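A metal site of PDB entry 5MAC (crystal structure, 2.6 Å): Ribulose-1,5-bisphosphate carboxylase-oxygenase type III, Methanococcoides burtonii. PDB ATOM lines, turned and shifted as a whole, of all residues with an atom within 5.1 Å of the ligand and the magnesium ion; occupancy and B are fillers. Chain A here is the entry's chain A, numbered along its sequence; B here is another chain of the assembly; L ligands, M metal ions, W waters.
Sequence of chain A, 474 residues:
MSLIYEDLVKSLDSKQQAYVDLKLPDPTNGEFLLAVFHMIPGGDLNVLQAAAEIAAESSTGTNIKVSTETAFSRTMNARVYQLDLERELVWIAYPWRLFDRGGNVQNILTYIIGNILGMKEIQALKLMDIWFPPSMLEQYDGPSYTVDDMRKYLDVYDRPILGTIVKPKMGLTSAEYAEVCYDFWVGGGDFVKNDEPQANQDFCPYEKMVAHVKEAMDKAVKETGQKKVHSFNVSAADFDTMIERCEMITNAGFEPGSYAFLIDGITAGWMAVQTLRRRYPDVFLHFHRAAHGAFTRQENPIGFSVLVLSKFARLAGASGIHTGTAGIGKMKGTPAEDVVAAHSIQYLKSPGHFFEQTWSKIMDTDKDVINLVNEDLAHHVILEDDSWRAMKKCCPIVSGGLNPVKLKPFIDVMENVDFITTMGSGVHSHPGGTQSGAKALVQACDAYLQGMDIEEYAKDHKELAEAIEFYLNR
CD1 of Ile 165 touches O8 of the ligand, 3.6 Å away.
Met 331 touches the ligand (CG to O12, 3.8 Å).
Met 423 touches the ligand.
Glu 57 of chain B touches the ligand.
Hydrophobic or aromatic side chains within 4 Å of the ligand: Ile 165, His 288, His 322 and Met 331.
20 residues have an atom within 4 Å of the ligand: Ile 165, Lys 167, Lys 169, KCX 193, Asp 195, Glu 196, His 288, Arg 289, His 322, Lys 330, Met 331, Ser 399, Gly 400, Gly 401, Met 423, Gly 424, Ser 425, Glu 57 of chain B, Thr 62 of chain B and Asn 115 of chain B.
The nearest printed residue that does not touch the ligand is Thr 422 (4.1 Å).
The side-chain carboxylate (OE2) of Glu 196 lies within hydrogen-bond range of the side-chain amide nitrogen (ND2) of Asn 115 of chain B (3.0 Å).
OE2 of Glu 196 lies within salt-bridge range of NZ of Lys 169, at 2.8 Å.
OD2 of Asp 195 is in salt-bridge range of NZ of Lys 167, at 2.7 Å.
OE2 of Glu 57 of chain B is in salt-bridge range of NZ of Lys 330, at 2.8 Å.
The guanidinium group (NE) of Arg 289 sits at hydrogen-bond distance from a ring nitrogen (NE2) of His 292 (3.3 Å).
The side-chain hydroxyl (OG) of Ser 399 sits at hydrogen-bond distance from the side-chain hydroxyl (OG1) of Thr 422, at 3.1 Å.
OE1 of Glu 57 of chain B lies within salt-bridge range of NZ of Lys 169, at 3.9 Å.
The side-chain carboxylate (OE2) of Glu 57 of chain B lies within hydrogen-bond range of the backbone NH (N) of Asn 63 of chain B (3.3 Å).
NZ of Lys 167 touches the magnesium ion, 3.97 Å away.
Asn 115 of chain B touches the magnesium ion (ND2 to MG, 3.4 Å).
Within 4 Å of the magnesium ion: Lys 167, KCX 193, Asp 195, Glu 196 and Asn 115 of chain B.
Along chain A the residues within 4 Å of the magnesium ion span positions 167 to 196.
The magnesium ion is bound by an oxygen (O7) of the ligand, an oxygen (O2) of the ligand, the side-chain carboxylate (OE1) of Glu 196, an oxygen (O3) of the ligand, the side-chain carboxylate (OD1) of Asp 195 and OQ2 of KCX 193.
The magnesium ion has six donor atoms within binding distance.
Water W5 lies within hydrogen-bond range of an oxygen (O13) of the ligand (2.6 Å), the backbone NH of Arg 289 (2.9 Å), a ring nitrogen (NE2) of His 288 (3.0 Å) and a ring nitrogen (ND1) of His 322 (3.3 Å).
Water W2 lies within hydrogen-bond range of the backbone carbonyl oxygen (O) of Leu 402 (2.6 Å), an oxygen (O8) of the ligand (2.7 Å), the backbone NH (N) of Gly 426 (2.7 Å), the side-chain hydroxyl (OG) of Ser 425 (3.1 Å) and the backbone NH (N) of Gly 424 (3.4 Å).
Water W9 bridges a ring nitrogen (NE2) of His 292 (2.7 Å) and an oxygen (O12) of the ligand (2.8 Å).
Water W3 lies within hydrogen-bond range of the backbone carbonyl oxygen of Ser 399 and an oxygen (O12) of the ligand.
Water W1 lies within hydrogen-bond range of the side-chain amide oxygen (OD1) of Asn 115 of chain B, an oxygen (O13) of the ligand and a ring nitrogen (NE2) of His 292.
Water W6 lies within hydrogen-bond range of NZ of Lys 169, OE1 of Glu 57 of chain B, O6 of the ligand and ND2 of Asn 115 of chain B.
An oxygen (O3) of the ligand sits close to a ring nitrogen (NE2) of His 288 (2.6 Å).
An oxygen (O9) of the ligand lies within hydrogen-bond range of the side-chain hydroxyl (OG1) of Thr 62 of chain B (2.7 Å).
NZ of Lys 330 lies within salt-bridge range of O10 of the ligand (2.7 Å).
O10 of the ligand is in hydrogen-bond range of N of Gly 401 (2.8 Å).
O4 of the ligand is in hydrogen-bond range of N of Gly 400, 2.9 Å away.
N of Gly 424 sits at hydrogen-bond distance from O8 of the ligand.
A ring nitrogen (ND1) of His 322 sits at hydrogen-bond distance from an oxygen (O11) of the ligand, at 2.9 Å.
O12 of the ligand is in salt-bridge range of NH2 of Arg 289 (2.9 Å).
The backbone NH (N) of Ser 425 is in hydrogen-bond range of an oxygen (O9) of the ligand.
ND2 of Asn 115 of chain B lies close to O3 of the ligand (3.1 Å).
O of Ser 399 lies close to O4 of the ligand, at 3.4 Å.
O4 of the ligand lies close to OG of Ser 399 (3.2 Å).
The side-chain amino group (NZ) of Lys 167 is in salt-bridge range of an oxygen (O9) of the ligand (3.6 Å).
The side-chain amino group (NZ) of Lys 169 lies close to an oxygen (O7) of the ligand, 3.3 Å away.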
ATOM      1  N   ILE A 165      19.641  21.725  13.629  1.00  0.00           N
ATOM      2  CA  ILE A 165      20.780  21.345  12.808  1.00  0.00           C
ATOM      3  C   ILE A 165      20.130  20.630  11.643  1.00  0.00           C
ATOM      4  O   ILE A 165      19.175  19.883  11.840  1.00  0.00           O
ATOM      5  CB  ILE A 165      21.754  20.387  13.533  1.00  0.00           C
ATOM      6  CG1 ILE A 165      22.079  20.815  14.963  1.00  0.00           C
ATOM      7  CG2 ILE A 165      23.013  20.225  12.701  1.00  0.00           C
ATOM      8  CD1 ILE A 165      21.298  20.054  16.019  1.00  0.00           C
ATOM      9  N   LYS A 167      19.641  17.785   9.129  1.00  0.00           N
ATOM     10  CA  LYS A 167      19.865  16.342   9.098  1.00  0.00           C
ATOM     11  C   LYS A 167      19.215  15.739   7.839  1.00  0.00           C
ATOM     12  O   LYS A 167      18.159  16.219   7.443  1.00  0.00           O
ATOM     13  CB  LYS A 167      19.253  15.691  10.343  1.00  0.00           C
ATOM     14  CG  LYS A 167      19.791  16.213  11.658  1.00  0.00           C
ATOM     15  CD  LYS A 167      21.248  15.860  11.928  1.00  0.00           C
ATOM     16  CE  LYS A 167      21.738  16.472  13.214  1.00  0.00           C
ATOM     17  NZ  LYS A 167      23.029  15.913  13.666  1.00  0.00           N
ATOM     18  N   LYS A 169      23.167  14.280   8.488  1.00  0.00           N
ATOM     19  CA  LYS A 169      24.471  14.903   8.752  1.00  0.00           C
ATOM     20  C   LYS A 169      25.272  15.104   7.449  1.00  0.00           C
ATOM     21  O   LYS A 169      26.058  16.049   7.334  1.00  0.00           O
ATOM     22  CB  LYS A 169      25.259  14.065   9.760  1.00  0.00           C
ATOM     23  CG  LYS A 169      26.688  14.534  10.029  1.00  0.00           C
ATOM     24  CD  LYS A 169      27.344  13.687  11.097  1.00  0.00           C
ATOM     25  CE  LYS A 169      26.668  13.825  12.406  1.00  0.00           C
ATOM     26  NZ  LYS A 169      27.622  13.886  13.534  1.00  0.00           N
ATOM     27  N   KCX A 193      21.596  25.733  11.991  1.00  0.00           N
ATOM     28  CA  KCX A 193      23.047  25.564  11.951  1.00  0.00           C
ATOM     29  CB  KCX A 193      23.761  25.357  13.318  1.00  0.00           C
ATOM     30  CG  KCX A 193      23.441  24.033  14.000  1.00  0.00           C
ATOM     31  CD  KCX A 193      24.229  23.876  15.302  1.00  0.00           C
ATOM     32  CE  KCX A 193      25.707  23.591  14.946  1.00  0.00           C
ATOM     33  NZ  KCX A 193      25.977  22.244  14.341  1.00  0.00           N
ATOM     34  C   KCX A 193      23.434  24.435  11.000  1.00  0.00           C
ATOM     35  O   KCX A 193      22.691  23.450  10.839  1.00  0.00           O
ATOM     36  CX  KCX A 193      25.927  21.059  15.046  1.00  0.00           C
ATOM     37  OQ1 KCX A 193      25.665  21.010  16.219  1.00  0.00           O
ATOM     38  OQ2 KCX A 193      26.148  19.913  14.443  1.00  0.00           O
ATOM     39  N   ASP A 195      25.272  21.141  10.240  1.00  0.00           N
ATOM     40  CA  ASP A 195      25.887  20.048  11.025  1.00  0.00           C
ATOM     41  C   ASP A 195      27.420  20.175  10.811  1.00  0.00           C
ATOM     42  O   ASP A 195      27.862  20.461   9.697  1.00  0.00           O
ATOM     43  CB  ASP A 195      25.372  18.661  10.591  1.00  0.00           C
ATOM     44  CG  ASP A 195      25.238  17.655  11.696  1.00  0.00           C
ATOM     45  OD1 ASP A 195      25.917  17.808  12.728  1.00  0.00           O
ATOM     46  OD2 ASP A 195      24.459  16.719  11.546  1.00  0.00           O
ATOM     47  N   GLU A 196      28.218  20.047  11.885  1.00  0.00           N
ATOM     48  CA  GLU A 196      29.675  20.295  11.877  1.00  0.00           C
ATOM     49  C   GLU A 196      30.484  19.823  10.642  1.00  0.00           C
ATOM     50  O   GLU A 196      31.463  20.510  10.354  1.00  0.00           O
ATOM     51  CB  GLU A 196      30.370  19.755  13.138  1.00  0.00           C
ATOM     52  CG  GLU A 196      30.411  18.256  13.312  1.00  0.00           C
ATOM     53  CD  GLU A 196      29.103  17.576  13.660  1.00  0.00           C
ATOM     54  OE1 GLU A 196      28.184  18.263  14.161  1.00  0.00           O
ATOM     55  OE2 GLU A 196      28.997  16.357  13.431  1.00  0.00           O
ATOM     56  N   HIS A 288      31.980  25.017  17.454  1.00  0.00           N
ATOM     57  CA  HIS A 288      31.590  23.635  17.535  1.00  0.00           C
ATOM     58  C   HIS A 288      32.862  22.926  18.113  1.00  0.00           C
ATOM     59  O   HIS A 288      33.986  23.320  17.762  1.00  0.00           O
ATOM     60  CB  HIS A 288      31.156  23.046  16.173  1.00  0.00           C
ATOM     61  CG  HIS A 288      30.375  21.796  16.360  1.00  0.00           C
ATOM     62  ND1 HIS A 288      30.993  20.569  16.482  1.00  0.00           N
ATOM     63  CD2 HIS A 288      29.041  21.632  16.570  1.00  0.00           C
ATOM     64  CE1 HIS A 288      30.020  19.703  16.714  1.00  0.00           C
ATOM     65  NE2 HIS A 288      28.842  20.301  16.801  1.00  0.00           N
ATOM     66  N   ARG A 289      32.675  21.950  19.039  1.00  0.00           N
ATOM     67  CA  ARG A 289      33.762  21.303  19.791  1.00  0.00           C
ATOM     68  C   ARG A 289      33.976  19.805  19.463  1.00  0.00           C
ATOM     69  O   ARG A 289      34.598  19.090  20.249  1.00  0.00           O
ATOM     70  CB  ARG A 289      33.544  21.512  21.337  1.00  0.00           C
ATOM     71  CG  ARG A 289      32.214  20.978  21.867  1.00  0.00           C
ATOM     72  CD  ARG A 289      32.144  21.049  23.380  1.00  0.00           C
ATOM     73  NE  ARG A 289      30.997  20.282  23.888  1.00  0.00           N
ATOM     74  CZ  ARG A 289      30.775  20.003  25.161  1.00  0.00           C
ATOM     75  NH1 ARG A 289      31.599  20.465  26.102  1.00  0.00           N
ATOM     76  NH2 ARG A 289      29.731  19.280  25.519  1.00  0.00           N
ATOM     77  N   HIS A 292      36.545  17.019  21.365  1.00  0.00           N
ATOM     78  CA  HIS A 292      36.899  17.456  22.727  1.00  0.00           C
ATOM     79  C   HIS A 292      36.927  16.304  23.757  1.00  0.00           C
ATOM     80  O   HIS A 292      37.641  16.406  24.768  1.00  0.00           O
ATOM     81  CB  HIS A 292      35.942  18.578  23.197  1.00  0.00           C
ATOM     82  CG  HIS A 292      34.564  18.106  23.549  1.00  0.00           C
ATOM     83  ND1 HIS A 292      34.227  17.803  24.852  1.00  0.00           N
ATOM     84  CD2 HIS A 292      33.490  17.858  22.768  1.00  0.00           C
ATOM     85  CE1 HIS A 292      32.972  17.369  24.803  1.00  0.00           C
ATOM     86  NE2 HIS A 292      32.501  17.393  23.571  1.00  0.00           N
ATOM     87  N   HIS A 322      29.549  25.164  22.497  1.00  0.00           N
ATOM     88  CA  HIS A 322      28.755  24.046  22.973  1.00  0.00           C
ATOM     89  C   HIS A 322      29.262  23.669  24.359  1.00  0.00           C
ATOM     90  O   HIS A 322      30.462  23.637  24.595  1.00  0.00           O
ATOM     91  CB  HIS A 322      28.834  22.860  22.023  1.00  0.00           C
ATOM     92  CG  HIS A 322      28.087  23.027  20.734  1.00  0.00           C
ATOM     93  ND1 HIS A 322      27.030  22.198  20.423  1.00  0.00           N
ATOM     94  CD2 HIS A 322      28.257  23.899  19.734  1.00  0.00           C
ATOM     95  CE1 HIS A 322      26.583  22.605  19.240  1.00  0.00           C
ATOM     96  NE2 HIS A 322      27.292  23.630  18.789  1.00  0.00           N
ATOM     97  N   GLY A 324      27.049  21.265  26.406  1.00  0.00           N
ATOM     98  CA  GLY A 324      26.393  20.020  26.733  1.00  0.00           C
ATOM     99  C   GLY A 324      25.043  20.150  27.418  1.00  0.00           C
ATOM    100  O   GLY A 324      24.703  21.195  27.958  1.00  0.00           O
ATOM    101  N   LYS A 330      22.261  12.670  24.489  1.00  0.00           N
ATOM    102  CA  LYS A 330      23.145  11.561  24.087  1.00  0.00           C
ATOM    103  C   LYS A 330      24.650  11.700  24.405  1.00  0.00           C
ATOM    104  O   LYS A 330      25.401  10.748  24.144  1.00  0.00           O
ATOM    105  CB  LYS A 330      22.984  11.309  22.568  1.00  0.00           C
ATOM    106  CG  LYS A 330      23.819  12.195  21.638  1.00  0.00           C
ATOM    107  CD  LYS A 330      23.320  12.078  20.239  1.00  0.00           C
ATOM    108  CE  LYS A 330      24.022  13.007  19.283  1.00  0.00           C
ATOM    109  NZ  LYS A 330      23.331  13.055  17.978  1.00  0.00           N
ATOM    110  N   MET A 331      25.105  12.854  24.953  1.00  0.00           N
ATOM    111  CA  MET A 331      26.533  13.043  25.278  1.00  0.00           C
ATOM    112  C   MET A 331      26.760  13.018  26.770  1.00  0.00           C
ATOM    113  O   MET A 331      25.835  13.219  27.550  1.00  0.00           O
ATOM    114  CB  MET A 331      27.074  14.357  24.685  1.00  0.00           C
ATOM    115  CG  MET A 331      26.838  14.531  23.206  1.00  0.00           C
ATOM    116  SD  MET A 331      27.784  13.400  22.165  1.00  0.00           S
ATOM    117  CE  MET A 331      27.251  13.880  20.586  1.00  0.00           C
ATOM    118  N   ILE A 397      25.777  26.816  23.871  1.00  0.00           N
ATOM    119  CA  ILE A 397      24.964  26.209  22.801  1.00  0.00           C
ATOM    120  C   ILE A 397      24.641  24.794  23.331  1.00  0.00           C
ATOM    121  O   ILE A 397      25.543  24.067  23.689  1.00  0.00           O
ATOM    122  CB  ILE A 397      25.670  26.220  21.437  1.00  0.00           C
ATOM    123  CG1 ILE A 397      26.075  27.696  21.089  1.00  0.00           C
ATOM    124  CG2 ILE A 397      24.736  25.662  20.358  1.00  0.00           C
ATOM    125  CD1 ILE A 397      26.963  27.899  19.942  1.00  0.00           C
ATOM    126  N   SER A 399      23.183  21.290  22.756  1.00  0.00           N
ATOM    127  CA  SER A 399      22.866  20.368  21.689  1.00  0.00           C
ATOM    128  C   SER A 399      23.229  18.954  22.092  1.00  0.00           C
ATOM    129  O   SER A 399      23.973  18.787  23.048  1.00  0.00           O
ATOM    130  CB  SER A 399      23.679  20.788  20.461  1.00  0.00           C
ATOM    131  OG  SER A 399      23.217  20.213  19.255  1.00  0.00           O
ATOM    132  N   GLY A 400      22.728  17.961  21.339  1.00  0.00           N
ATOM    133  CA  GLY A 400      23.018  16.535  21.536  1.00  0.00           C
ATOM    134  C   GLY A 400      21.903  15.628  22.047  1.00  0.00           C
ATOM    135  O   GLY A 400      21.877  15.284  23.208  1.00  0.00           O
ATOM    136  N   GLY A 401      21.046  15.174  21.160  1.00  0.00           N
ATOM    137  CA  GLY A 401      20.010  14.200  21.470  1.00  0.00           C
ATOM    138  C   GLY A 401      18.853  14.702  22.291  1.00  0.00           C
ATOM    139  O   GLY A 401      18.236  13.921  23.019  1.00  0.00           O
ATOM    140  N   LEU A 402      18.496  15.974  22.114  1.00  0.00           N
ATOM    141  CA  LEU A 402      17.366  16.591  22.827  1.00  0.00           C
ATOM    142  C   LEU A 402      16.143  16.567  21.962  1.00  0.00           C
ATOM    143  O   LEU A 402      16.271  16.643  20.746  1.00  0.00           O
ATOM    144  CB  LEU A 402      17.661  18.045  23.103  1.00  0.00           C
ATOM    145  CG  LEU A 402      18.846  18.348  23.980  1.00  0.00           C
ATOM    146  CD1 LEU A 402      19.326  19.769  23.732  1.00  0.00           C
ATOM    147  CD2 LEU A 402      18.517  18.096  25.437  1.00  0.00           C
ATOM    148  N   THR A 422      19.832  23.613  20.043  1.00  0.00           N
ATOM    149  CA  THR A 422      19.635  23.057  18.716  1.00  0.00           C
ATOM    150  C   THR A 422      19.210  21.618  18.847  1.00  0.00           C
ATOM    151  O   THR A 422      19.830  20.846  19.576  1.00  0.00           O
ATOM    152  CB  THR A 422      20.845  23.285  17.804  1.00  0.00           C
ATOM    153  OG1 THR A 422      22.037  22.952  18.478  1.00  0.00           O
ATOM    154  CG2 THR A 422      20.914  24.700  17.295  1.00  0.00           C
ATOM    155  N   MET A 423      18.106  21.289  18.187  1.00  0.00           N
ATOM    156  CA  MET A 423      17.543  19.955  18.129  1.00  0.00           C
ATOM    157  C   MET A 423      17.428  19.502  16.649  1.00  0.00           C
ATOM    158  O   MET A 423      16.615  20.034  15.906  1.00  0.00           O
ATOM    159  CB  MET A 423      16.180  19.970  18.827  1.00  0.00           C
ATOM    160  CG  MET A 423      16.260  20.568  20.157  1.00  0.00           C
ATOM    161  SD  MET A 423      14.786  20.153  21.100  1.00  0.00           S
ATOM    162  CE  MET A 423      15.280  20.740  22.706  1.00  0.00           C
ATOM    163  N   GLY A 424      18.288  18.556  16.247  1.00  0.00           N
ATOM    164  CA  GLY A 424      18.272  17.984  14.892  1.00  0.00           C
ATOM    165  C   GLY A 424      17.320  16.800  14.842  1.00  0.00           C
ATOM    166  O   GLY A 424      16.237  16.903  14.259  1.00  0.00           O
ATOM    167  N   SER A 425      17.689  15.688  15.485  1.00  0.00           N
ATOM    168  CA  SER A 425      16.826  14.492  15.532  1.00  0.00           C
ATOM    169  C   SER A 425      15.513  14.791  16.282  1.00  0.00           C
ATOM    170  O   SER A 425      14.463  14.306  15.876  1.00  0.00           O
ATOM    171  CB  SER A 425      17.570  13.296  16.142  1.00  0.00           C
ATOM    172  OG  SER A 425      17.754  13.397  17.543  1.00  0.00           O
ATOM    173  N   GLY A 426      15.549  15.665  17.281  1.00  0.00           N
ATOM    174  CA  GLY A 426      14.355  16.057  18.022  1.00  0.00           C
ATOM    175  C   GLY A 426      13.376  16.931  17.258  1.00  0.00           C
ATOM    176  O   GLY A 426      12.375  17.349  17.832  1.00  0.00           O
ATOM    177  N   GLU B  57      26.589   8.379  13.723  1.00  0.00           N
ATOM    178  CA  GLU B  57      27.067   9.678  14.166  1.00  0.00           C
ATOM    179  C   GLU B  57      28.366  10.156  13.520  1.00  0.00           C
ATOM    180  O   GLU B  57      28.642  11.341  13.569  1.00  0.00           O
ATOM    181  CB  GLU B  57      27.190   9.679  15.674  1.00  0.00           C
ATOM    182  CG  GLU B  57      25.858   9.478  16.364  1.00  0.00           C
ATOM    183  CD  GLU B  57      24.896  10.628  16.316  1.00  0.00           C
ATOM    184  OE1 GLU B  57      25.221  11.673  15.730  1.00  0.00           O
ATOM    185  OE2 GLU B  57      23.797  10.477  16.911  1.00  0.00           O
ATOM    186  N   THR B  62      21.846  10.175  12.788  1.00  0.00           N
ATOM    187  CA  THR B  62      21.612  10.732  14.106  1.00  0.00           C
ATOM    188  C   THR B  62      20.844   9.765  14.997  1.00  0.00           C
ATOM    189  O   THR B  62      20.501   8.684  14.573  1.00  0.00           O
ATOM    190  CB  THR B  62      20.973  12.100  13.979  1.00  0.00           C
ATOM    191  OG1 THR B  62      21.015  12.730  15.295  1.00  0.00           O
ATOM    192  CG2 THR B  62      19.571  12.018  13.351  1.00  0.00           C
ATOM    193  N   ASN B  63      20.611  10.171  16.252  1.00  0.00           N
ATOM    194  CA  ASN B  63      20.011   9.372  17.317  1.00  0.00           C
ATOM    195  C   ASN B  63      18.663   8.652  16.949  1.00  0.00           C
ATOM    196  O   ASN B  63      18.392   7.554  17.449  1.00  0.00           O
ATOM    197  CB  ASN B  63      19.834  10.251  18.581  1.00  0.00           C
ATOM    198  CG  ASN B  63      19.639   9.455  19.814  1.00  0.00           C
ATOM    199  OD1 ASN B  63      18.551   9.443  20.411  1.00  0.00           O
ATOM    200  ND2 ASN B  63      20.709   8.749  20.218  1.00  0.00           N
ATOM    201  N   ASN B 115      32.472  14.026  17.279  1.00  0.00           N
ATOM    202  CA  ASN B 115      31.328  13.916  18.192  1.00  0.00           C
ATOM    203  C   ASN B 115      31.203  12.573  18.866  1.00  0.00           C
ATOM    204  O   ASN B 115      30.817  12.518  20.025  1.00  0.00           O
ATOM    205  CB  ASN B 115      30.013  14.255  17.469  1.00  0.00           C
ATOM    206  CG  ASN B 115      29.715  15.736  17.332  1.00  0.00           C
ATOM    207  OD1 ASN B 115      30.256  16.576  18.069  1.00  0.00           O
ATOM    208  ND2 ASN B 115      28.793  16.077  16.445  1.00  0.00           N
HETATM  209  C1  LIG L   1      23.387  17.326  17.548  1.00  0.00           C
HETATM  210  C2  LIG L   1      24.760  17.401  16.866  1.00  0.00           C
HETATM  211  C3  LIG L   1      25.803  18.186  17.682  1.00  0.00           C
HETATM  212  C4  LIG L   1      26.242  17.598  19.030  1.00  0.00           C
HETATM  213  C5  LIG L   1      27.553  18.190  19.499  1.00  0.00           C
HETATM  214  C6  LIG L   1      25.301  16.038  16.461  1.00  0.00           C
HETATM  215  O1  LIG L   1      22.417  16.716  16.707  1.00  0.00           O
HETATM  216  O2  LIG L   1      24.508  18.133  15.665  1.00  0.00           O
HETATM  217  O3  LIG L   1      26.933  18.493  16.852  1.00  0.00           O
HETATM  218  O4  LIG L   1      25.269  17.875  20.025  1.00  0.00           O
HETATM  219  O5  LIG L   1      27.805  17.742  20.832  1.00  0.00           O
HETATM  220  O6  LIG L   1      25.199  15.030  17.197  1.00  0.00           O
HETATM  221  O7  LIG L   1      25.870  15.941  15.352  1.00  0.00           O
HETATM  222  P1  LIG L   1      21.108  15.998  17.326  1.00  0.00           P
HETATM  223  P2  LIG L   1      28.129  18.827  21.958  1.00  0.00           P
HETATM  224  O8  LIG L   1      20.241  17.151  17.808  1.00  0.00           O
HETATM  225  O9  LIG L   1      20.511  15.224  16.181  1.00  0.00           O
HETATM  226  O10 LIG L   1      21.573  15.079  18.416  1.00  0.00           O
HETATM  227  O11 LIG L   1      26.884  19.688  21.930  1.00  0.00           O
HETATM  228  O12 LIG L   1      28.276  18.080  23.260  1.00  0.00           O
HETATM  229  O13 LIG L   1      29.434  19.453  21.479  1.00  0.00           O
HETATM  230 MG    MG M   1      26.319  17.764  14.893  1.00  0.00          MG
HETATM  231  O   HOH W   1      31.158  17.429  20.523  1.00  0.00           O
HETATM  232  O   HOH W   2      17.822  16.260  18.685  1.00  0.00           O
HETATM  233  O   HOH W   3      25.802  17.330  24.366  1.00  0.00           O
HETATM  234  O   HOH W   4      19.976  18.218  20.139  1.00  0.00           O
HETATM  235  O   HOH W   5      30.004  21.042  19.493  1.00  0.00           O
HETATM  236  O   HOH W   6      27.397  13.316  16.160  1.00  0.00           O
HETATM  237  O   HOH W   7      23.944  13.457  14.138  1.00  0.00           O
HETATM  238  O   HOH W   8      26.055  21.556  23.653  1.00  0.00           O
HETATM  239  O   HOH W   9      30.152  16.060  23.672  1.00  0.00           O
